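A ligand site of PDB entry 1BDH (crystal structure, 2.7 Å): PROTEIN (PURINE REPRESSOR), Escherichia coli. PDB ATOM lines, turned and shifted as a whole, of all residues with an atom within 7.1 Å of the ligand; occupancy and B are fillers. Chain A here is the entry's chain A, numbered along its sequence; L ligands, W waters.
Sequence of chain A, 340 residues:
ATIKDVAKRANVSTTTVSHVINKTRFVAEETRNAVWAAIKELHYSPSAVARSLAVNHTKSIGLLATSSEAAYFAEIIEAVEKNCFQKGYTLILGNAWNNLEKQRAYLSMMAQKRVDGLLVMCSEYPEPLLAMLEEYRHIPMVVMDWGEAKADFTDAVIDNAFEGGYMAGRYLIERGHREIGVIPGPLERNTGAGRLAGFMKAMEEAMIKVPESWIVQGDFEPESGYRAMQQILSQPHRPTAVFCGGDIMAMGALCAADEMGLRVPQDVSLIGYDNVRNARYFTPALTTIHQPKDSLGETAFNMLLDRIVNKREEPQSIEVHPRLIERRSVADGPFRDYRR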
ATOM      1  N   THR A  66      14.779 -10.642  30.031  1.00  0.00           N
ATOM      2  CA  THR A  66      14.514 -10.002  28.762  1.00  0.00           C
ATOM      3  C   THR A  66      13.468  -8.939  29.001  1.00  0.00           C
ATOM      4  O   THR A  66      13.721  -7.764  28.845  1.00  0.00           O
ATOM      5  CB  THR A  66      13.927 -11.057  27.860  1.00  0.00           C
ATOM      6  OG1 THR A  66      14.839 -12.161  27.790  1.00  0.00           O
ATOM      7  CG2 THR A  66      13.671 -10.524  26.510  1.00  0.00           C
ATOM      8  N   SER A  67      12.301  -9.393  29.419  1.00  0.00           N
ATOM      9  CA  SER A  67      11.150  -8.525  29.716  1.00  0.00           C
ATOM     10  C   SER A  67      10.358  -9.240  30.829  1.00  0.00           C
ATOM     11  O   SER A  67      10.531 -10.423  31.074  1.00  0.00           O
ATOM     12  CB  SER A  67      10.336  -8.274  28.390  1.00  0.00           C
ATOM     13  OG  SER A  67       8.959  -8.621  28.430  1.00  0.00           O
ATOM     14  N   ALA A  70       5.085  -9.847  29.846  1.00  0.00           N
ATOM     15  CA  ALA A  70       4.664 -11.015  29.104  1.00  0.00           C
ATOM     16  C   ALA A  70       4.346 -12.157  30.030  1.00  0.00           C
ATOM     17  O   ALA A  70       5.162 -12.565  30.878  1.00  0.00           O
ATOM     18  CB  ALA A  70       5.805 -11.419  28.158  1.00  0.00           C
ATOM     19  N   ALA A  71       3.117 -12.653  29.860  1.00  0.00           N
ATOM     20  CA  ALA A  71       2.602 -13.748  30.661  1.00  0.00           C
ATOM     21  C   ALA A  71       3.614 -14.821  30.898  1.00  0.00           C
ATOM     22  O   ALA A  71       3.903 -15.175  32.050  1.00  0.00           O
ATOM     23  CB  ALA A  71       1.376 -14.361  29.959  1.00  0.00           C
ATOM     24  N   TYR A  72       4.140 -15.346  29.789  1.00  0.00           N
ATOM     25  CA  TYR A  72       5.113 -16.407  29.847  1.00  0.00           C
ATOM     26  C   TYR A  72       6.193 -16.049  30.846  1.00  0.00           C
ATOM     27  O   TYR A  72       6.404 -16.744  31.820  1.00  0.00           O
ATOM     28  CB  TYR A  72       5.677 -16.623  28.467  1.00  0.00           C
ATOM     29  CG  TYR A  72       6.707 -17.729  28.372  1.00  0.00           C
ATOM     30  CD1 TYR A  72       6.324 -19.065  28.363  1.00  0.00           C
ATOM     31  CD2 TYR A  72       8.044 -17.447  28.235  1.00  0.00           C
ATOM     32  CE1 TYR A  72       7.253 -20.093  28.259  1.00  0.00           C
ATOM     33  CE2 TYR A  72       8.974 -18.449  28.104  1.00  0.00           C
ATOM     34  CZ  TYR A  72       8.582 -19.777  28.138  1.00  0.00           C
ATOM     35  OH  TYR A  72       9.541 -20.765  28.014  1.00  0.00           O
ATOM     36  N   PHE A  73       6.827 -14.926  30.628  1.00  0.00           N
ATOM     37  CA  PHE A  73       7.879 -14.471  31.508  1.00  0.00           C
ATOM     38  C   PHE A  73       7.408 -14.258  32.881  1.00  0.00           C
ATOM     39  O   PHE A  73       7.963 -14.762  33.848  1.00  0.00           O
ATOM     40  CB  PHE A  73       8.450 -13.168  30.997  1.00  0.00           C
ATOM     41  CG  PHE A  73       9.237 -13.362  29.754  1.00  0.00           C
ATOM     42  CD1 PHE A  73       9.850 -14.559  29.538  1.00  0.00           C
ATOM     43  CD2 PHE A  73       9.339 -12.383  28.801  1.00  0.00           C
ATOM     44  CE1 PHE A  73      10.574 -14.752  28.385  1.00  0.00           C
ATOM     45  CE2 PHE A  73      10.044 -12.583  27.622  1.00  0.00           C
ATOM     46  CZ  PHE A  73      10.671 -13.757  27.414  1.00  0.00           C
ATOM     47  N   SER A 123      16.663 -14.874  26.003  1.00  0.00           N
ATOM     48  CA  SER A 123      15.960 -15.149  24.760  1.00  0.00           C
ATOM     49  C   SER A 123      16.848 -15.335  23.601  1.00  0.00           C
ATOM     50  O   SER A 123      16.871 -16.405  23.062  1.00  0.00           O
ATOM     51  CB  SER A 123      14.902 -14.082  24.465  1.00  0.00           C
ATOM     52  OG  SER A 123      13.954 -14.053  25.535  1.00  0.00           O
ATOM     53  N   ASP A 145      16.931 -20.621  29.223  1.00  0.00           N
ATOM     54  CA  ASP A 145      16.193 -20.666  27.964  1.00  0.00           C
ATOM     55  C   ASP A 145      16.764 -21.230  26.680  1.00  0.00           C
ATOM     56  O   ASP A 145      16.299 -20.885  25.587  1.00  0.00           O
ATOM     57  CB  ASP A 145      15.513 -19.344  27.716  1.00  0.00           C
ATOM     58  CG  ASP A 145      16.474 -18.177  27.745  1.00  0.00           C
ATOM     59  OD1 ASP A 145      17.705 -18.422  27.644  1.00  0.00           O
ATOM     60  OD2 ASP A 145      15.967 -17.017  27.770  1.00  0.00           O
ATOM     61  N   PRO A 186      10.040 -15.776  17.009  1.00  0.00           N
ATOM     62  CA  PRO A 186      11.405 -15.453  16.552  1.00  0.00           C
ATOM     63  C   PRO A 186      12.360 -16.654  16.438  1.00  0.00           C
ATOM     64  O   PRO A 186      12.637 -17.362  17.412  1.00  0.00           O
ATOM     65  CB  PRO A 186      11.892 -14.522  17.657  1.00  0.00           C
ATOM     66  CG  PRO A 186      10.635 -13.956  18.249  1.00  0.00           C
ATOM     67  CD  PRO A 186       9.672 -15.058  18.235  1.00  0.00           C
ATOM     68  N   ARG A 189      15.268 -17.714  18.676  1.00  0.00           N
ATOM     69  CA  ARG A 189      14.955 -18.214  19.990  1.00  0.00           C
ATOM     70  C   ARG A 189      14.631 -19.687  19.979  1.00  0.00           C
ATOM     71  O   ARG A 189      14.117 -20.235  19.007  1.00  0.00           O
ATOM     72  CB  ARG A 189      13.692 -17.548  20.465  1.00  0.00           C
ATOM     73  CG  ARG A 189      13.947 -16.477  21.372  1.00  0.00           C
ATOM     74  CD  ARG A 189      13.348 -15.330  20.769  1.00  0.00           C
ATOM     75  NE  ARG A 189      12.402 -14.774  21.702  1.00  0.00           N
ATOM     76  CZ  ARG A 189      12.374 -13.479  21.937  1.00  0.00           C
ATOM     77  NH1 ARG A 189      13.236 -12.714  21.294  1.00  0.00           N
ATOM     78  NH2 ARG A 189      11.519 -12.947  22.803  1.00  0.00           N
ATOM     79  N   ASN A 190      14.879 -20.316  21.109  1.00  0.00           N
ATOM     80  CA  ASN A 190      14.605 -21.725  21.290  1.00  0.00           C
ATOM     81  C   ASN A 190      13.109 -21.953  21.066  1.00  0.00           C
ATOM     82  O   ASN A 190      12.696 -22.708  20.131  1.00  0.00           O
ATOM     83  CB  ASN A 190      14.949 -22.110  22.711  1.00  0.00           C
ATOM     84  CG  ASN A 190      14.680 -23.536  22.959  1.00  0.00           C
ATOM     85  OD1 ASN A 190      14.938 -24.382  22.079  1.00  0.00           O
ATOM     86  ND2 ASN A 190      14.005 -23.808  24.067  1.00  0.00           N
ATOM     87  N   THR A 191      12.309 -21.292  21.932  1.00  0.00           N
ATOM     88  CA  THR A 191      10.842 -21.351  21.872  1.00  0.00           C
ATOM     89  C   THR A 191      10.328 -20.926  20.484  1.00  0.00           C
ATOM     90  O   THR A 191       9.163 -21.145  20.178  1.00  0.00           O
ATOM     91  CB  THR A 191      10.204 -20.432  22.913  1.00  0.00           C
ATOM     92  OG1 THR A 191      10.740 -19.115  22.749  1.00  0.00           O
ATOM     93  CG2 THR A 191      10.485 -20.904  24.348  1.00  0.00           C
ATOM     94  N   GLY A 192      11.176 -20.336  19.639  1.00  0.00           N
ATOM     95  CA  GLY A 192      10.772 -19.954  18.286  1.00  0.00           C
ATOM     96  C   GLY A 192      11.198 -21.117  17.368  1.00  0.00           C
ATOM     97  O   GLY A 192      10.445 -22.014  17.035  1.00  0.00           O
ATOM     98  N   ARG A 195      10.355 -24.942  18.344  1.00  0.00           N
ATOM     99  CA  ARG A 195       9.009 -25.441  18.375  1.00  0.00           C
ATOM    100  C   ARG A 195       8.593 -25.719  16.956  1.00  0.00           C
ATOM    101  O   ARG A 195       7.956 -26.730  16.660  1.00  0.00           O
ATOM    102  CB  ARG A 195       8.061 -24.454  19.106  1.00  0.00           C
ATOM    103  CG  ARG A 195       8.287 -24.325  20.653  1.00  0.00           C
ATOM    104  CD  ARG A 195       7.474 -23.138  21.333  1.00  0.00           C
ATOM    105  NE  ARG A 195       7.608 -23.014  22.801  1.00  0.00           N
ATOM    106  CZ  ARG A 195       6.953 -22.133  23.560  1.00  0.00           C
ATOM    107  NH1 ARG A 195       6.102 -21.283  22.995  1.00  0.00           N
ATOM    108  NH2 ARG A 195       7.161 -22.092  24.880  1.00  0.00           N
ATOM    109  N   ASP A 219       6.124 -12.433  16.934  1.00  0.00           N
ATOM    110  CA  ASP A 219       7.176 -11.956  17.824  1.00  0.00           C
ATOM    111  C   ASP A 219       6.769 -12.254  19.269  1.00  0.00           C
ATOM    112  O   ASP A 219       7.314 -11.640  20.193  1.00  0.00           O
ATOM    113  CB  ASP A 219       7.332 -10.439  17.631  1.00  0.00           C
ATOM    114  CG  ASP A 219       6.061  -9.677  17.977  1.00  0.00           C
ATOM    115  OD1 ASP A 219       5.174 -10.136  18.727  1.00  0.00           O
ATOM    116  OD2 ASP A 219       5.947  -8.542  17.507  1.00  0.00           O
ATOM    117  N   PHE A 220       5.784 -13.128  19.436  1.00  0.00           N
ATOM    118  CA  PHE A 220       5.143 -13.535  20.721  1.00  0.00           C
ATOM    119  C   PHE A 220       4.160 -12.528  21.262  1.00  0.00           C
ATOM    120  O   PHE A 220       3.659 -12.709  22.375  1.00  0.00           O
ATOM    121  CB  PHE A 220       6.085 -13.890  21.867  1.00  0.00           C
ATOM    122  CG  PHE A 220       6.775 -15.185  21.683  1.00  0.00           C
ATOM    123  CD1 PHE A 220       6.046 -16.343  21.623  1.00  0.00           C
ATOM    124  CD2 PHE A 220       8.154 -15.242  21.518  1.00  0.00           C
ATOM    125  CE1 PHE A 220       6.685 -17.531  21.438  1.00  0.00           C
ATOM    126  CE2 PHE A 220       8.784 -16.413  21.324  1.00  0.00           C
ATOM    127  CZ  PHE A 220       8.044 -17.566  21.294  1.00  0.00           C
ATOM    128  N   GLU A 221       3.888 -11.467  20.511  1.00  0.00           N
ATOM    129  CA  GLU A 221       2.958 -10.460  20.978  1.00  0.00           C
ATOM    130  C   GLU A 221       1.626 -10.518  20.231  1.00  0.00           C
ATOM    131  O   GLU A 221       1.557 -10.759  19.013  1.00  0.00           O
ATOM    132  CB  GLU A 221       3.598  -9.091  20.859  1.00  0.00           C
ATOM    133  CG  GLU A 221       4.855  -8.959  21.704  1.00  0.00           C
ATOM    134  CD  GLU A 221       4.550  -8.390  23.070  1.00  0.00           C
ATOM    135  OE1 GLU A 221       4.165  -9.176  23.966  1.00  0.00           O
ATOM    136  OE2 GLU A 221       4.667  -7.153  23.244  1.00  0.00           O
ATOM    137  N   GLY A 245       2.666 -20.648  17.740  1.00  0.00           N
ATOM    138  CA  GLY A 245       3.796 -20.739  18.667  1.00  0.00           C
ATOM    139  C   GLY A 245       3.820 -20.227  20.082  1.00  0.00           C
ATOM    140  O   GLY A 245       4.766 -20.474  20.794  1.00  0.00           O
ATOM    141  N   GLY A 246       2.821 -19.485  20.493  1.00  0.00           N
ATOM    142  CA  GLY A 246       2.738 -18.925  21.848  1.00  0.00           C
ATOM    143  C   GLY A 246       1.282 -18.570  22.157  1.00  0.00           C
ATOM    144  O   GLY A 246       0.530 -18.008  21.325  1.00  0.00           O
ATOM    145  N   ASP A 247       0.836 -18.902  23.353  1.00  0.00           N
ATOM    146  CA  ASP A 247      -0.540 -18.560  23.660  1.00  0.00           C
ATOM    147  C   ASP A 247      -0.964 -17.062  23.430  1.00  0.00           C
ATOM    148  O   ASP A 247      -2.048 -16.751  22.908  1.00  0.00           O
ATOM    149  CB  ASP A 247      -0.870 -19.033  25.058  1.00  0.00           C
ATOM    150  CG  ASP A 247      -0.870 -20.555  25.191  1.00  0.00           C
ATOM    151  OD1 ASP A 247      -0.672 -21.268  24.188  1.00  0.00           O
ATOM    152  OD2 ASP A 247      -1.154 -21.051  26.301  1.00  0.00           O
ATOM    153  N   ILE A 248      -0.108 -16.126  23.796  1.00  0.00           N
ATOM    154  CA  ILE A 248      -0.491 -14.731  23.596  1.00  0.00           C
ATOM    155  C   ILE A 248      -0.711 -14.326  22.152  1.00  0.00           C
ATOM    156  O   ILE A 248      -1.662 -13.625  21.818  1.00  0.00           O
ATOM    157  CB  ILE A 248       0.448 -13.748  24.255  1.00  0.00           C
ATOM    158  CG1 ILE A 248       0.696 -14.138  25.706  1.00  0.00           C
ATOM    159  CG2 ILE A 248      -0.190 -12.351  24.204  1.00  0.00           C
ATOM    160  CD1 ILE A 248      -0.514 -13.881  26.518  1.00  0.00           C
ATOM    161  N   TYR A 273       0.573 -22.654  22.327  1.00  0.00           N
ATOM    162  CA  TYR A 273       1.712 -23.200  23.030  1.00  0.00           C
ATOM    163  C   TYR A 273       2.182 -22.346  24.170  1.00  0.00           C
ATOM    164  O   TYR A 273       2.518 -21.171  23.914  1.00  0.00           O
ATOM    165  CB  TYR A 273       2.868 -23.314  22.086  1.00  0.00           C
ATOM    166  CG  TYR A 273       3.909 -24.294  22.569  1.00  0.00           C
ATOM    167  CD1 TYR A 273       4.409 -24.257  23.867  1.00  0.00           C
ATOM    168  CD2 TYR A 273       4.418 -25.271  21.714  1.00  0.00           C
ATOM    169  CE1 TYR A 273       5.380 -25.156  24.277  1.00  0.00           C
ATOM    170  CE2 TYR A 273       5.402 -26.160  22.121  1.00  0.00           C
ATOM    171  CZ  TYR A 273       5.882 -26.110  23.389  1.00  0.00           C
ATOM    172  OH  TYR A 273       6.847 -27.018  23.759  1.00  0.00           O
ATOM    173  N   ASP A 274       2.189 -22.943  25.382  1.00  0.00           N
ATOM    174  CA  ASP A 274       2.636 -22.364  26.650  1.00  0.00           C
ATOM    175  C   ASP A 274       1.766 -22.720  27.799  1.00  0.00           C
ATOM    176  O   ASP A 274       2.229 -22.934  28.938  1.00  0.00           O
ATOM    177  CB  ASP A 274       2.701 -20.816  26.611  1.00  0.00           C
ATOM    178  CG  ASP A 274       4.015 -20.274  25.990  1.00  0.00           C
ATOM    179  OD1 ASP A 274       4.852 -21.075  25.529  1.00  0.00           O
ATOM    180  OD2 ASP A 274       4.126 -19.051  25.788  1.00  0.00           O
ATOM    181  N   VAL A 276      -0.511 -20.688  29.248  1.00  0.00           N
ATOM    182  CA  VAL A 276      -0.363 -19.585  30.171  1.00  0.00           C
ATOM    183  C   VAL A 276      -1.539 -19.620  31.144  1.00  0.00           C
ATOM    184  O   VAL A 276      -2.615 -20.074  30.795  1.00  0.00           O
ATOM    185  CB  VAL A 276      -0.358 -18.286  29.383  1.00  0.00           C
ATOM    186  CG1 VAL A 276      -1.057 -17.219  30.174  1.00  0.00           C
ATOM    187  CG2 VAL A 276       1.084 -17.893  29.023  1.00  0.00           C
ATOM    188  N   GLN A 291       3.807 -25.718  29.085  1.00  0.00           N
ATOM    189  CA  GLN A 291       5.237 -25.632  29.453  1.00  0.00           C
ATOM    190  C   GLN A 291       5.255 -25.548  30.939  1.00  0.00           C
ATOM    191  O   GLN A 291       4.569 -24.699  31.505  1.00  0.00           O
ATOM    192  CB  GLN A 291       5.914 -24.345  29.009  1.00  0.00           C
ATOM    193  CG  GLN A 291       7.380 -24.248  29.464  1.00  0.00           C
ATOM    194  CD  GLN A 291       8.345 -24.683  28.355  1.00  0.00           C
ATOM    195  OE1 GLN A 291       9.235 -23.902  27.930  1.00  0.00           O
ATOM    196  NE2 GLN A 291       8.145 -25.907  27.832  1.00  0.00           N
HETATM  197  N1  LIG L   1       8.375 -14.396  24.857  1.00  0.00           N
HETATM  198  C1  LIG L   1       7.082 -14.423  25.319  1.00  0.00           C
HETATM  199  N2  LIG L   1       6.385 -15.527  25.514  1.00  0.00           N
HETATM  200  C2  LIG L   1       7.109 -16.620  25.192  1.00  0.00           C
HETATM  201  C3  LIG L   1       8.399 -16.688  24.714  1.00  0.00           C
HETATM  202  C4  LIG L   1       9.143 -15.505  24.533  1.00  0.00           C
HETATM  203  O1  LIG L   1      10.315 -15.321  24.150  1.00  0.00           O
HETATM  204  N3  LIG L   1       8.745 -18.011  24.480  1.00  0.00           N
HETATM  205  C5  LIG L   1       7.700 -18.698  24.842  1.00  0.00           C
HETATM  206  N4  LIG L   1       6.659 -17.913  25.279  1.00  0.00           N
HETATM  207  O   HOH W   1       3.748 -14.585  26.530  1.00  0.00           O
HETATM  208  O   HOH W   2       9.260 -11.382  24.109  1.00  0.00           O
HETATM  209  O   HOH W   3      11.725 -18.525  25.820  1.00  0.00           O
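N4 of the ligand is in hydrogen-bond range of OD2 of Asp 274 (2.8 Å). OG1 of Thr 191 sits at hydrogen-bond distance from N3 of the ligand, 2.9 Å away. The guanidinium group of Arg 189 is in hydrogen-bond range of an oxygen (O1) of the ligand (3.0 Å).
OE1 of Gln 291 sits at hydrogen-bond distance from OH of Tyr 72 (3.2 Å). OD1 of Asp 274 is in salt-bridge range of NH2 of Arg 195 (2.6 Å). O of Gly 245 sits at hydrogen-bond distance from NH1 of Arg 195, at 2.7 Å. The backbone carbonyl oxygen (O) of Asp 274 lies within hydrogen-bond range of the backbone NH (N) of Gln 291, at 3.2 Å.
Tyr 72 touches the ligand. Phe 73 touches the ligand. NH2 of Arg 195 touches C5 of the ligand, at 3.4 Å. CD2 of Phe 220 touches C4 of the ligand, at 3.2 Å. Of the 25 residues printed, 7 come within 4 Å of the ligand. The nearest printed residue that does not touch the ligand is Ser 123 (4.1 Å).
Water W1 bridges N2 of the ligand and N of Tyr 72. Water W2 bridges the guanidinium group of Arg 189 (3.0 Å) and a nitrogen (N1) of the ligand (3.2 Å). Water W3 bridges the side-chain hydroxyl of Thr 191 (3.3 Å) and a nitrogen (N3) of the ligand (3.3 Å).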
